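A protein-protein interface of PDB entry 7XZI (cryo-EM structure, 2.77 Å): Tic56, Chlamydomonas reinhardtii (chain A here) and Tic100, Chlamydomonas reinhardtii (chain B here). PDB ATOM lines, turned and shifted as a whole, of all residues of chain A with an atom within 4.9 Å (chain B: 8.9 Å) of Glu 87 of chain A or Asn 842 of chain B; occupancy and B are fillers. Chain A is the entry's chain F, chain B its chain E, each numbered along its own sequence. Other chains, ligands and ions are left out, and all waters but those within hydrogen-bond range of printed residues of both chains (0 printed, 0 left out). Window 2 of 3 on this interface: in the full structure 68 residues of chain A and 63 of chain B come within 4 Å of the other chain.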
ATOM      1  N   LEU A  83     -22.792  27.294 -31.438  1.00  0.00           N
ATOM      2  CA  LEU A  83     -23.455  26.036 -31.112  1.00  0.00           C
ATOM      3  C   LEU A  83     -23.876  25.999 -29.648  1.00  0.00           C
ATOM      4  O   LEU A  83     -24.969  25.525 -29.321  1.00  0.00           O
ATOM      5  CB  LEU A  83     -22.535  24.859 -31.440  1.00  0.00           C
ATOM      6  CG  LEU A  83     -23.102  23.456 -31.219  1.00  0.00           C
ATOM      7  CD1 LEU A  83     -24.356  23.248 -32.053  1.00  0.00           C
ATOM      8  CD2 LEU A  83     -22.060  22.394 -31.539  1.00  0.00           C
ATOM      9  N   ALA A  84     -23.019  26.495 -28.753  1.00  0.00           N
ATOM     10  CA  ALA A  84     -23.361  26.529 -27.334  1.00  0.00           C
ATOM     11  C   ALA A  84     -24.556  27.438 -27.076  1.00  0.00           C
ATOM     12  O   ALA A  84     -25.452  27.099 -26.294  1.00  0.00           O
ATOM     13  CB  ALA A  84     -22.151  26.978 -26.515  1.00  0.00           C
ATOM     14  N   GLN A  85     -24.585  28.606 -27.721  1.00  0.00           N
ATOM     15  CA  GLN A  85     -25.717  29.513 -27.551  1.00  0.00           C
ATOM     16  C   GLN A  85     -27.002  28.898 -28.095  1.00  0.00           C
ATOM     17  O   GLN A  85     -28.069  29.026 -27.480  1.00  0.00           O
ATOM     18  CB  GLN A  85     -25.431  30.852 -28.231  1.00  0.00           C
ATOM     19  CG  GLN A  85     -24.296  31.640 -27.597  1.00  0.00           C
ATOM     20  CD  GLN A  85     -24.092  32.995 -28.248  1.00  0.00           C
ATOM     21  OE1 GLN A  85     -24.944  33.471 -28.998  1.00  0.00           O
ATOM     22  NE2 GLN A  85     -22.958  33.624 -27.963  1.00  0.00           N
ATOM     23  N   MET A  86     -26.921  28.227 -29.246  1.00  0.00           N
ATOM     24  CA  MET A  86     -28.096  27.562 -29.800  1.00  0.00           C
ATOM     25  C   MET A  86     -28.586  26.450 -28.881  1.00  0.00           C
ATOM     26  O   MET A  86     -29.796  26.271 -28.701  1.00  0.00           O
ATOM     27  CB  MET A  86     -27.785  27.014 -31.191  1.00  0.00           C
ATOM     28  CG  MET A  86     -27.539  28.088 -32.240  1.00  0.00           C
ATOM     29  SD  MET A  86     -28.983  29.132 -32.507  1.00  0.00           S
ATOM     30  CE  MET A  86     -30.187  27.908 -33.015  1.00  0.00           C
ATOM     31  N   GLU A  87     -27.661  25.687 -28.294  1.00  0.00           N
ATOM     32  CA  GLU A  87     -28.052  24.627 -27.370  1.00  0.00           C
ATOM     33  C   GLU A  87     -28.681  25.200 -26.105  1.00  0.00           C
ATOM     34  O   GLU A  87     -29.630  24.624 -25.566  1.00  0.00           O
ATOM     35  CB  GLU A  87     -26.847  23.749 -27.030  1.00  0.00           C
ATOM     36  CG  GLU A  87     -26.378  22.881 -28.189  1.00  0.00           C
ATOM     37  CD  GLU A  87     -25.320  21.870 -27.783  1.00  0.00           C
ATOM     38  OE1 GLU A  87     -24.843  21.933 -26.631  1.00  0.00           O
ATOM     39  OE2 GLU A  87     -24.970  21.009 -28.618  1.00  0.00           O
ATOM     40  N   ALA A  88     -28.167  26.331 -25.615  1.00  0.00           N
ATOM     41  CA  ALA A  88     -28.792  26.987 -24.470  1.00  0.00           C
ATOM     42  C   ALA A  88     -30.200  27.464 -24.812  1.00  0.00           C
ATOM     43  O   ALA A  88     -31.127  27.323 -24.006  1.00  0.00           O
ATOM     44  CB  ALA A  88     -27.928  28.153 -23.996  1.00  0.00           C
ATOM     45  N   MET A  89     -30.377  28.029 -26.009  1.00  0.00           N
ATOM     46  CA  MET A  89     -31.706  28.453 -26.440  1.00  0.00           C
ATOM     47  C   MET A  89     -32.659  27.267 -26.544  1.00  0.00           C
ATOM     48  O   MET A  89     -33.833  27.368 -26.170  1.00  0.00           O
ATOM     49  CB  MET A  89     -31.612  29.184 -27.777  1.00  0.00           C
ATOM     50  CG  MET A  89     -30.929  30.538 -27.698  1.00  0.00           C
ATOM     51  SD  MET A  89     -30.603  31.228 -29.330  1.00  0.00           S
ATOM     52  CE  MET A  89     -32.218  31.088 -30.091  1.00  0.00           C
ATOM     53  N   GLU A  90     -32.173  26.138 -27.063  1.00  0.00           N
ATOM     54  CA  GLU A  90     -32.998  24.935 -27.138  1.00  0.00           C
ATOM     55  C   GLU A  90     -33.354  24.423 -25.747  1.00  0.00           C
ATOM     56  O   GLU A  90     -34.490  23.999 -25.504  1.00  0.00           O
ATOM     57  CB  GLU A  90     -32.273  23.856 -27.943  1.00  0.00           C
ATOM     58  CG  GLU A  90     -33.053  22.565 -28.110  1.00  0.00           C
ATOM     59  CD  GLU A  90     -32.324  21.558 -28.976  1.00  0.00           C
ATOM     60  OE1 GLU A  90     -31.190  21.856 -29.409  1.00  0.00           O
ATOM     61  OE2 GLU A  90     -32.882  20.470 -29.226  1.00  0.00           O
ATOM     62  N   LEU A  91     -32.392  24.450 -24.822  1.00  0.00           N
ATOM     63  CA  LEU A  91     -32.665  24.070 -23.439  1.00  0.00           C
ATOM     64  C   LEU A  91     -33.716  24.979 -22.819  1.00  0.00           C
ATOM     65  O   LEU A  91     -34.514  24.540 -21.983  1.00  0.00           O
ATOM     66  CB  LEU A  91     -31.377  24.114 -22.616  1.00  0.00           C
ATOM     67  CG  LEU A  91     -30.523  22.849 -22.560  1.00  0.00           C
ATOM     68  CD1 LEU A  91     -29.275  23.085 -21.725  1.00  0.00           C
ATOM     69  CD2 LEU A  91     -31.340  21.702 -21.996  1.00  0.00           C
ATOM     70  N   LEU B  13     -25.505   6.127 -28.158  1.00  0.00           N
ATOM     71  CA  LEU B  13     -25.351   6.222 -26.711  1.00  0.00           C
ATOM     72  C   LEU B  13     -26.346   5.312 -25.999  1.00  0.00           C
ATOM     73  O   LEU B  13     -27.364   4.924 -26.572  1.00  0.00           O
ATOM     74  CB  LEU B  13     -25.530   7.668 -26.239  1.00  0.00           C
ATOM     75  CG  LEU B  13     -24.560   8.724 -26.778  1.00  0.00           C
ATOM     76  CD1 LEU B  13     -25.053   9.316 -28.094  1.00  0.00           C
ATOM     77  CD2 LEU B  13     -24.331   9.819 -25.748  1.00  0.00           C
ATOM     78  N   ARG B 834     -34.528  12.482 -23.217  1.00  0.00           N
ATOM     79  CA  ARG B 834     -33.213  12.088 -23.715  1.00  0.00           C
ATOM     80  C   ARG B 834     -32.460  13.280 -24.297  1.00  0.00           C
ATOM     81  O   ARG B 834     -31.244  13.418 -24.098  1.00  0.00           O
ATOM     82  CB  ARG B 834     -33.354  10.976 -24.753  1.00  0.00           C
ATOM     83  CG  ARG B 834     -33.668   9.613 -24.157  1.00  0.00           C
ATOM     84  CD  ARG B 834     -33.606   8.516 -25.207  1.00  0.00           C
ATOM     85  NE  ARG B 834     -34.785   8.499 -26.058  1.00  0.00           N
ATOM     86  CZ  ARG B 834     -35.842   7.719 -25.858  1.00  0.00           C
ATOM     87  NH1 ARG B 834     -35.891   6.870 -24.845  1.00  0.00           N
ATOM     88  NH2 ARG B 834     -36.871   7.794 -26.695  1.00  0.00           N
ATOM     89  N   ARG B 835     -33.166  14.154 -25.019  1.00  0.00           N
ATOM     90  CA  ARG B 835     -32.534  15.357 -25.548  1.00  0.00           C
ATOM     91  C   ARG B 835     -32.020  16.246 -24.425  1.00  0.00           C
ATOM     92  O   ARG B 835     -30.931  16.822 -24.527  1.00  0.00           O
ATOM     93  CB  ARG B 835     -33.520  16.125 -26.425  1.00  0.00           C
ATOM     94  CG  ARG B 835     -32.895  17.270 -27.196  1.00  0.00           C
ATOM     95  CD  ARG B 835     -32.012  16.746 -28.312  1.00  0.00           C
ATOM     96  NE  ARG B 835     -31.463  17.819 -29.125  1.00  0.00           N
ATOM     97  CZ  ARG B 835     -30.184  18.179 -29.131  1.00  0.00           C
ATOM     98  NH1 ARG B 835     -29.287  17.549 -28.391  1.00  0.00           N
ATOM     99  NH2 ARG B 835     -29.797  19.187 -29.906  1.00  0.00           N
ATOM    100  N   ALA B 836     -32.799  16.382 -23.349  1.00  0.00           N
ATOM    101  CA  ALA B 836     -32.368  17.183 -22.208  1.00  0.00           C
ATOM    102  C   ALA B 836     -31.098  16.616 -21.591  1.00  0.00           C
ATOM    103  O   ALA B 836     -30.162  17.359 -21.267  1.00  0.00           O
ATOM    104  CB  ALA B 836     -33.485  17.256 -21.168  1.00  0.00           C
ATOM    105  N   GLN B 837     -31.051  15.293 -21.418  1.00  0.00           N
ATOM    106  CA  GLN B 837     -29.851  14.677 -20.858  1.00  0.00           C
ATOM    107  C   GLN B 837     -28.642  14.915 -21.755  1.00  0.00           C
ATOM    108  O   GLN B 837     -27.550  15.244 -21.268  1.00  0.00           O
ATOM    109  CB  GLN B 837     -30.066  13.180 -20.645  1.00  0.00           C
ATOM    110  CG  GLN B 837     -28.959  12.528 -19.830  1.00  0.00           C
ATOM    111  CD  GLN B 837     -28.921  11.023 -19.986  1.00  0.00           C
ATOM    112  OE1 GLN B 837     -29.564  10.463 -20.873  1.00  0.00           O
ATOM    113  NE2 GLN B 837     -28.161  10.358 -19.124  1.00  0.00           N
ATOM    114  N   GLU B 838     -28.818  14.764 -23.070  1.00  0.00           N
ATOM    115  CA  GLU B 838     -27.703  14.973 -23.991  1.00  0.00           C
ATOM    116  C   GLU B 838     -27.218  16.418 -23.960  1.00  0.00           C
ATOM    117  O   GLU B 838     -26.006  16.678 -23.964  1.00  0.00           O
ATOM    118  CB  GLU B 838     -28.115  14.574 -25.407  1.00  0.00           C
ATOM    119  CG  GLU B 838     -26.991  14.649 -26.421  1.00  0.00           C
ATOM    120  CD  GLU B 838     -27.439  14.255 -27.813  1.00  0.00           C
ATOM    121  OE1 GLU B 838     -28.654  14.047 -28.010  1.00  0.00           O
ATOM    122  OE2 GLU B 838     -26.576  14.153 -28.710  1.00  0.00           O
ATOM    123  N   LEU B 839     -28.149  17.375 -23.934  1.00  0.00           N
ATOM    124  CA  LEU B 839     -27.766  18.783 -23.891  1.00  0.00           C
ATOM    125  C   LEU B 839     -27.026  19.116 -22.602  1.00  0.00           C
ATOM    126  O   LEU B 839     -26.029  19.849 -22.623  1.00  0.00           O
ATOM    127  CB  LEU B 839     -29.001  19.669 -24.047  1.00  0.00           C
ATOM    128  CG  LEU B 839     -29.633  19.682 -25.439  1.00  0.00           C
ATOM    129  CD1 LEU B 839     -30.878  20.550 -25.459  1.00  0.00           C
ATOM    130  CD2 LEU B 839     -28.624  20.163 -26.467  1.00  0.00           C
ATOM    131  N   ARG B 840     -27.498  18.591 -21.469  1.00  0.00           N
ATOM    132  CA  ARG B 840     -26.796  18.834 -20.213  1.00  0.00           C
ATOM    133  C   ARG B 840     -25.399  18.230 -20.242  1.00  0.00           C
ATOM    134  O   ARG B 840     -24.446  18.835 -19.738  1.00  0.00           O
ATOM    135  CB  ARG B 840     -27.588  18.280 -19.031  1.00  0.00           C
ATOM    136  CG  ARG B 840     -26.949  18.619 -17.694  1.00  0.00           C
ATOM    137  CD  ARG B 840     -27.524  17.795 -16.564  1.00  0.00           C
ATOM    138  NE  ARG B 840     -26.878  18.093 -15.294  1.00  0.00           N
ATOM    139  CZ  ARG B 840     -25.749  17.529 -14.876  1.00  0.00           C
ATOM    140  NH1 ARG B 840     -25.106  16.639 -15.613  1.00  0.00           N
ATOM    141  NH2 ARG B 840     -25.256  17.871 -13.690  1.00  0.00           N
ATOM    142  N   ASN B 841     -25.258  17.034 -20.820  1.00  0.00           N
ATOM    143  CA  ASN B 841     -23.934  16.426 -20.921  1.00  0.00           C
ATOM    144  C   ASN B 841     -22.999  17.270 -21.780  1.00  0.00           C
ATOM    145  O   ASN B 841     -21.826  17.455 -21.433  1.00  0.00           O
ATOM    146  CB  ASN B 841     -24.045  15.007 -21.476  1.00  0.00           C
ATOM    147  CG  ASN B 841     -24.516  14.010 -20.435  1.00  0.00           C
ATOM    148  OD1 ASN B 841     -25.106  14.385 -19.422  1.00  0.00           O
ATOM    149  ND2 ASN B 841     -24.254  12.730 -20.678  1.00  0.00           N
ATOM    150  N   ASN B 842     -23.498  17.794 -22.903  1.00  0.00           N
ATOM    151  CA  ASN B 842     -22.667  18.644 -23.755  1.00  0.00           C
ATOM    152  C   ASN B 842     -22.257  19.922 -23.026  1.00  0.00           C
ATOM    153  O   ASN B 842     -21.104  20.366 -23.119  1.00  0.00           O
ATOM    154  CB  ASN B 842     -23.403  18.977 -25.052  1.00  0.00           C
ATOM    155  CG  ASN B 842     -23.588  17.767 -25.945  1.00  0.00           C
ATOM    156  OD1 ASN B 842     -22.792  16.828 -25.912  1.00  0.00           O
ATOM    157  ND2 ASN B 842     -24.641  17.783 -26.752  1.00  0.00           N
ATOM    158  N   ALA B 843     -23.196  20.531 -22.299  1.00  0.00           N
ATOM    159  CA  ALA B 843     -22.877  21.737 -21.540  1.00  0.00           C
ATOM    160  C   ALA B 843     -21.827  21.455 -20.473  1.00  0.00           C
ATOM    161  O   ALA B 843     -20.896  22.247 -20.277  1.00  0.00           O
ATOM    162  CB  ALA B 843     -24.146  22.311 -20.911  1.00  0.00           C
ATOM    163  N   MET B 844     -21.960  20.327 -19.771  1.00  0.00           N
ATOM    164  CA  MET B 844     -20.977  19.966 -18.755  1.00  0.00           C
ATOM    165  C   MET B 844     -19.612  19.702 -19.378  1.00  0.00           C
ATOM    166  O   MET B 844     -18.580  20.048 -18.796  1.00  0.00           O
ATOM    167  CB  MET B 844     -21.453  18.747 -17.967  1.00  0.00           C
ATOM    168  CG  MET B 844     -20.602  18.437 -16.746  1.00  0.00           C
ATOM    169  SD  MET B 844     -21.126  16.950 -15.875  1.00  0.00           S
ATOM    170  CE  MET B 844     -20.860  15.706 -17.137  1.00  0.00           C
ATOM    171  N   ALA B 845     -19.587  19.081 -20.560  1.00  0.00           N
ATOM    172  CA  ALA B 845     -18.317  18.849 -21.243  1.00  0.00           C
ATOM    173  C   ALA B 845     -17.646  20.164 -21.622  1.00  0.00           C
ATOM    174  O   ALA B 845     -16.427  20.317 -21.470  1.00  0.00           O
ATOM    175  CB  ALA B 845     -18.536  17.980 -22.480  1.00  0.00           C
ATOM    176  N   ARG B 846     -18.426  21.128 -22.119  1.00  0.00           N
ATOM    177  CA  ARG B 846     -17.860  22.437 -22.438  1.00  0.00           C
ATOM    178  C   ARG B 846     -17.338  23.135 -21.186  1.00  0.00           C
ATOM    179  O   ARG B 846     -16.270  23.764 -21.212  1.00  0.00           O
ATOM    180  CB  ARG B 846     -18.898  23.307 -23.146  1.00  0.00           C
ATOM    181  CG  ARG B 846     -19.098  22.960 -24.612  1.00  0.00           C
ATOM    182  CD  ARG B 846     -19.942  24.005 -25.321  1.00  0.00           C
ATOM    183  NE  ARG B 846     -21.334  23.965 -24.901  1.00  0.00           N
ATOM    184  CZ  ARG B 846     -22.278  23.253 -25.506  1.00  0.00           C
ATOM    185  NH1 ARG B 846     -22.008  22.505 -26.563  1.00  0.00           N
ATOM    186  NH2 ARG B 846     -23.522  23.295 -25.040  1.00  0.00           N
ATOM    187  N   TYR B 847     -18.080  23.039 -20.080  1.00  0.00           N
ATOM    188  CA  TYR B 847     -17.612  23.622 -18.825  1.00  0.00           C
ATOM    189  C   TYR B 847     -16.314  22.971 -18.362  1.00  0.00           C
ATOM    190  O   TYR B 847     -15.408  23.653 -17.872  1.00  0.00           O
ATOM    191  CB  TYR B 847     -18.689  23.494 -17.748  1.00  0.00           C
ATOM    192  CG  TYR B 847     -19.362  24.800 -17.396  1.00  0.00           C
ATOM    193  CD1 TYR B 847     -18.823  25.643 -16.435  1.00  0.00           C
ATOM    194  CD2 TYR B 847     -20.535  25.189 -18.024  1.00  0.00           C
ATOM    195  CE1 TYR B 847     -19.435  26.836 -16.108  1.00  0.00           C
ATOM    196  CE2 TYR B 847     -21.155  26.381 -17.704  1.00  0.00           C
ATOM    197  CZ  TYR B 847     -20.600  27.201 -16.747  1.00  0.00           C
ATOM    198  OH  TYR B 847     -21.214  28.389 -16.426  1.00  0.00           O
ATOM    199  N   LEU B 848     -16.212  21.647 -18.500  1.00  0.00           N
ATOM    200  CA  LEU B 848     -14.983  20.951 -18.137  1.00  0.00           C
ATOM    201  C   LEU B 848     -13.819  21.391 -19.012  1.00  0.00           C
ATOM    202  O   LEU B 848     -12.691  21.543 -18.527  1.00  0.00           O
ATOM    203  CB  LEU B 848     -15.184  19.439 -18.236  1.00  0.00           C
ATOM    204  CG  LEU B 848     -15.837  18.753 -17.038  1.00  0.00           C
ATOM    205  CD1 LEU B 848     -16.018  17.268 -17.303  1.00  0.00           C
ATOM    206  CD2 LEU B 848     -15.000  18.978 -15.791  1.00  0.00           C
ATOM    207  N   ALA B 849     -14.066  21.582 -20.310  1.00  0.00           N
ATOM    208  CA  ALA B 849     -13.011  22.069 -21.194  1.00  0.00           C
ATOM    209  C   ALA B 849     -12.541  23.457 -20.774  1.00  0.00           C
ATOM    210  O   ALA B 849     -11.335  23.734 -20.744  1.00  0.00           O
ATOM    211  CB  ALA B 849     -13.503  22.080 -22.641  1.00  0.00           C
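Of the 17 printed residues of chain B, 4 touch a printed residue of chain A. Hydrophobic or aromatic side chains of chain B that line the printed part of chain A: Leu 839. Hydrophobic or aromatic side chains of chain A that line the printed part of chain B: Ala 84 and Leu 91. Among the printed residues, 7 pairs touch across the chains. Among the printed residues, Asp or Glu carboxylates within 4 Å of a Lys or Arg side-chain nitrogen of the other chain: Glu 87 of chain A with Arg 846 of chain B (2.5 Å) and Glu 90 of chain A with Arg 835 of chain B (3.0 Å).
Glu 87 of chain A touches three residues of chain B. No residue of chain B comes within 4 Å of Ala 88 of chain A. Of the printed residues of chain B, Leu 91 of chain A touches Leu 839 (3.7 Å). Of the printed residues of chain A, Arg 835 of chain B touches Glu 90. Of the printed residues of chain A, Leu 839 of chain B touches Glu 87, Glu 90 and Leu 91. Arg 840 of chain B touches none of the printed residues of chain A. Asn 842 of chain B touches just one residue of chain A: Glu 87 (3.6 Å). Leu 848 of chain B touches none of the printed residues of chain A. The nearest residue of chain B that does not touch Glu 87 of chain A is Ala 843 of chain B (4.8 Å). The nearest printed residue of chain A that does not touch Asn 842 of chain B is Leu 83 of chain A (7.1 Å).
The guanidinium group of Arg 835 of chain B lies within salt-bridge range of the side-chain carboxylate of Glu 90 of chain A. NH2 of Arg 846 of chain B lies within salt-bridge range of OE1 of Glu 87 of chain A, 2.5 Å away.
O of Glu 838 of chain B sits at hydrogen-bond distance from ND2 of Asn 842 of chain B (3.3 Å). The guanidinium group of Arg 835 of chain B lies within salt-bridge range of the side-chain carboxylate of Glu 838 of chain B (3.6 Å).
CB of Ala 84 of chain A touches NE of Arg 846 of chain B, 3.5 Å away. Glu 87 of chain A touches Leu 839 of chain B. OE1 of Glu 87 of chain A touches CB of Asn 842 of chain B, at 3.6 Å. Leu 839 of chain B touches Glu 90 of chain A (CD1 to CD, 3.9 Å). CD2 of Leu 91 of chain A touches CD1 of Leu 839 of chain B, at 3.7 Å.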
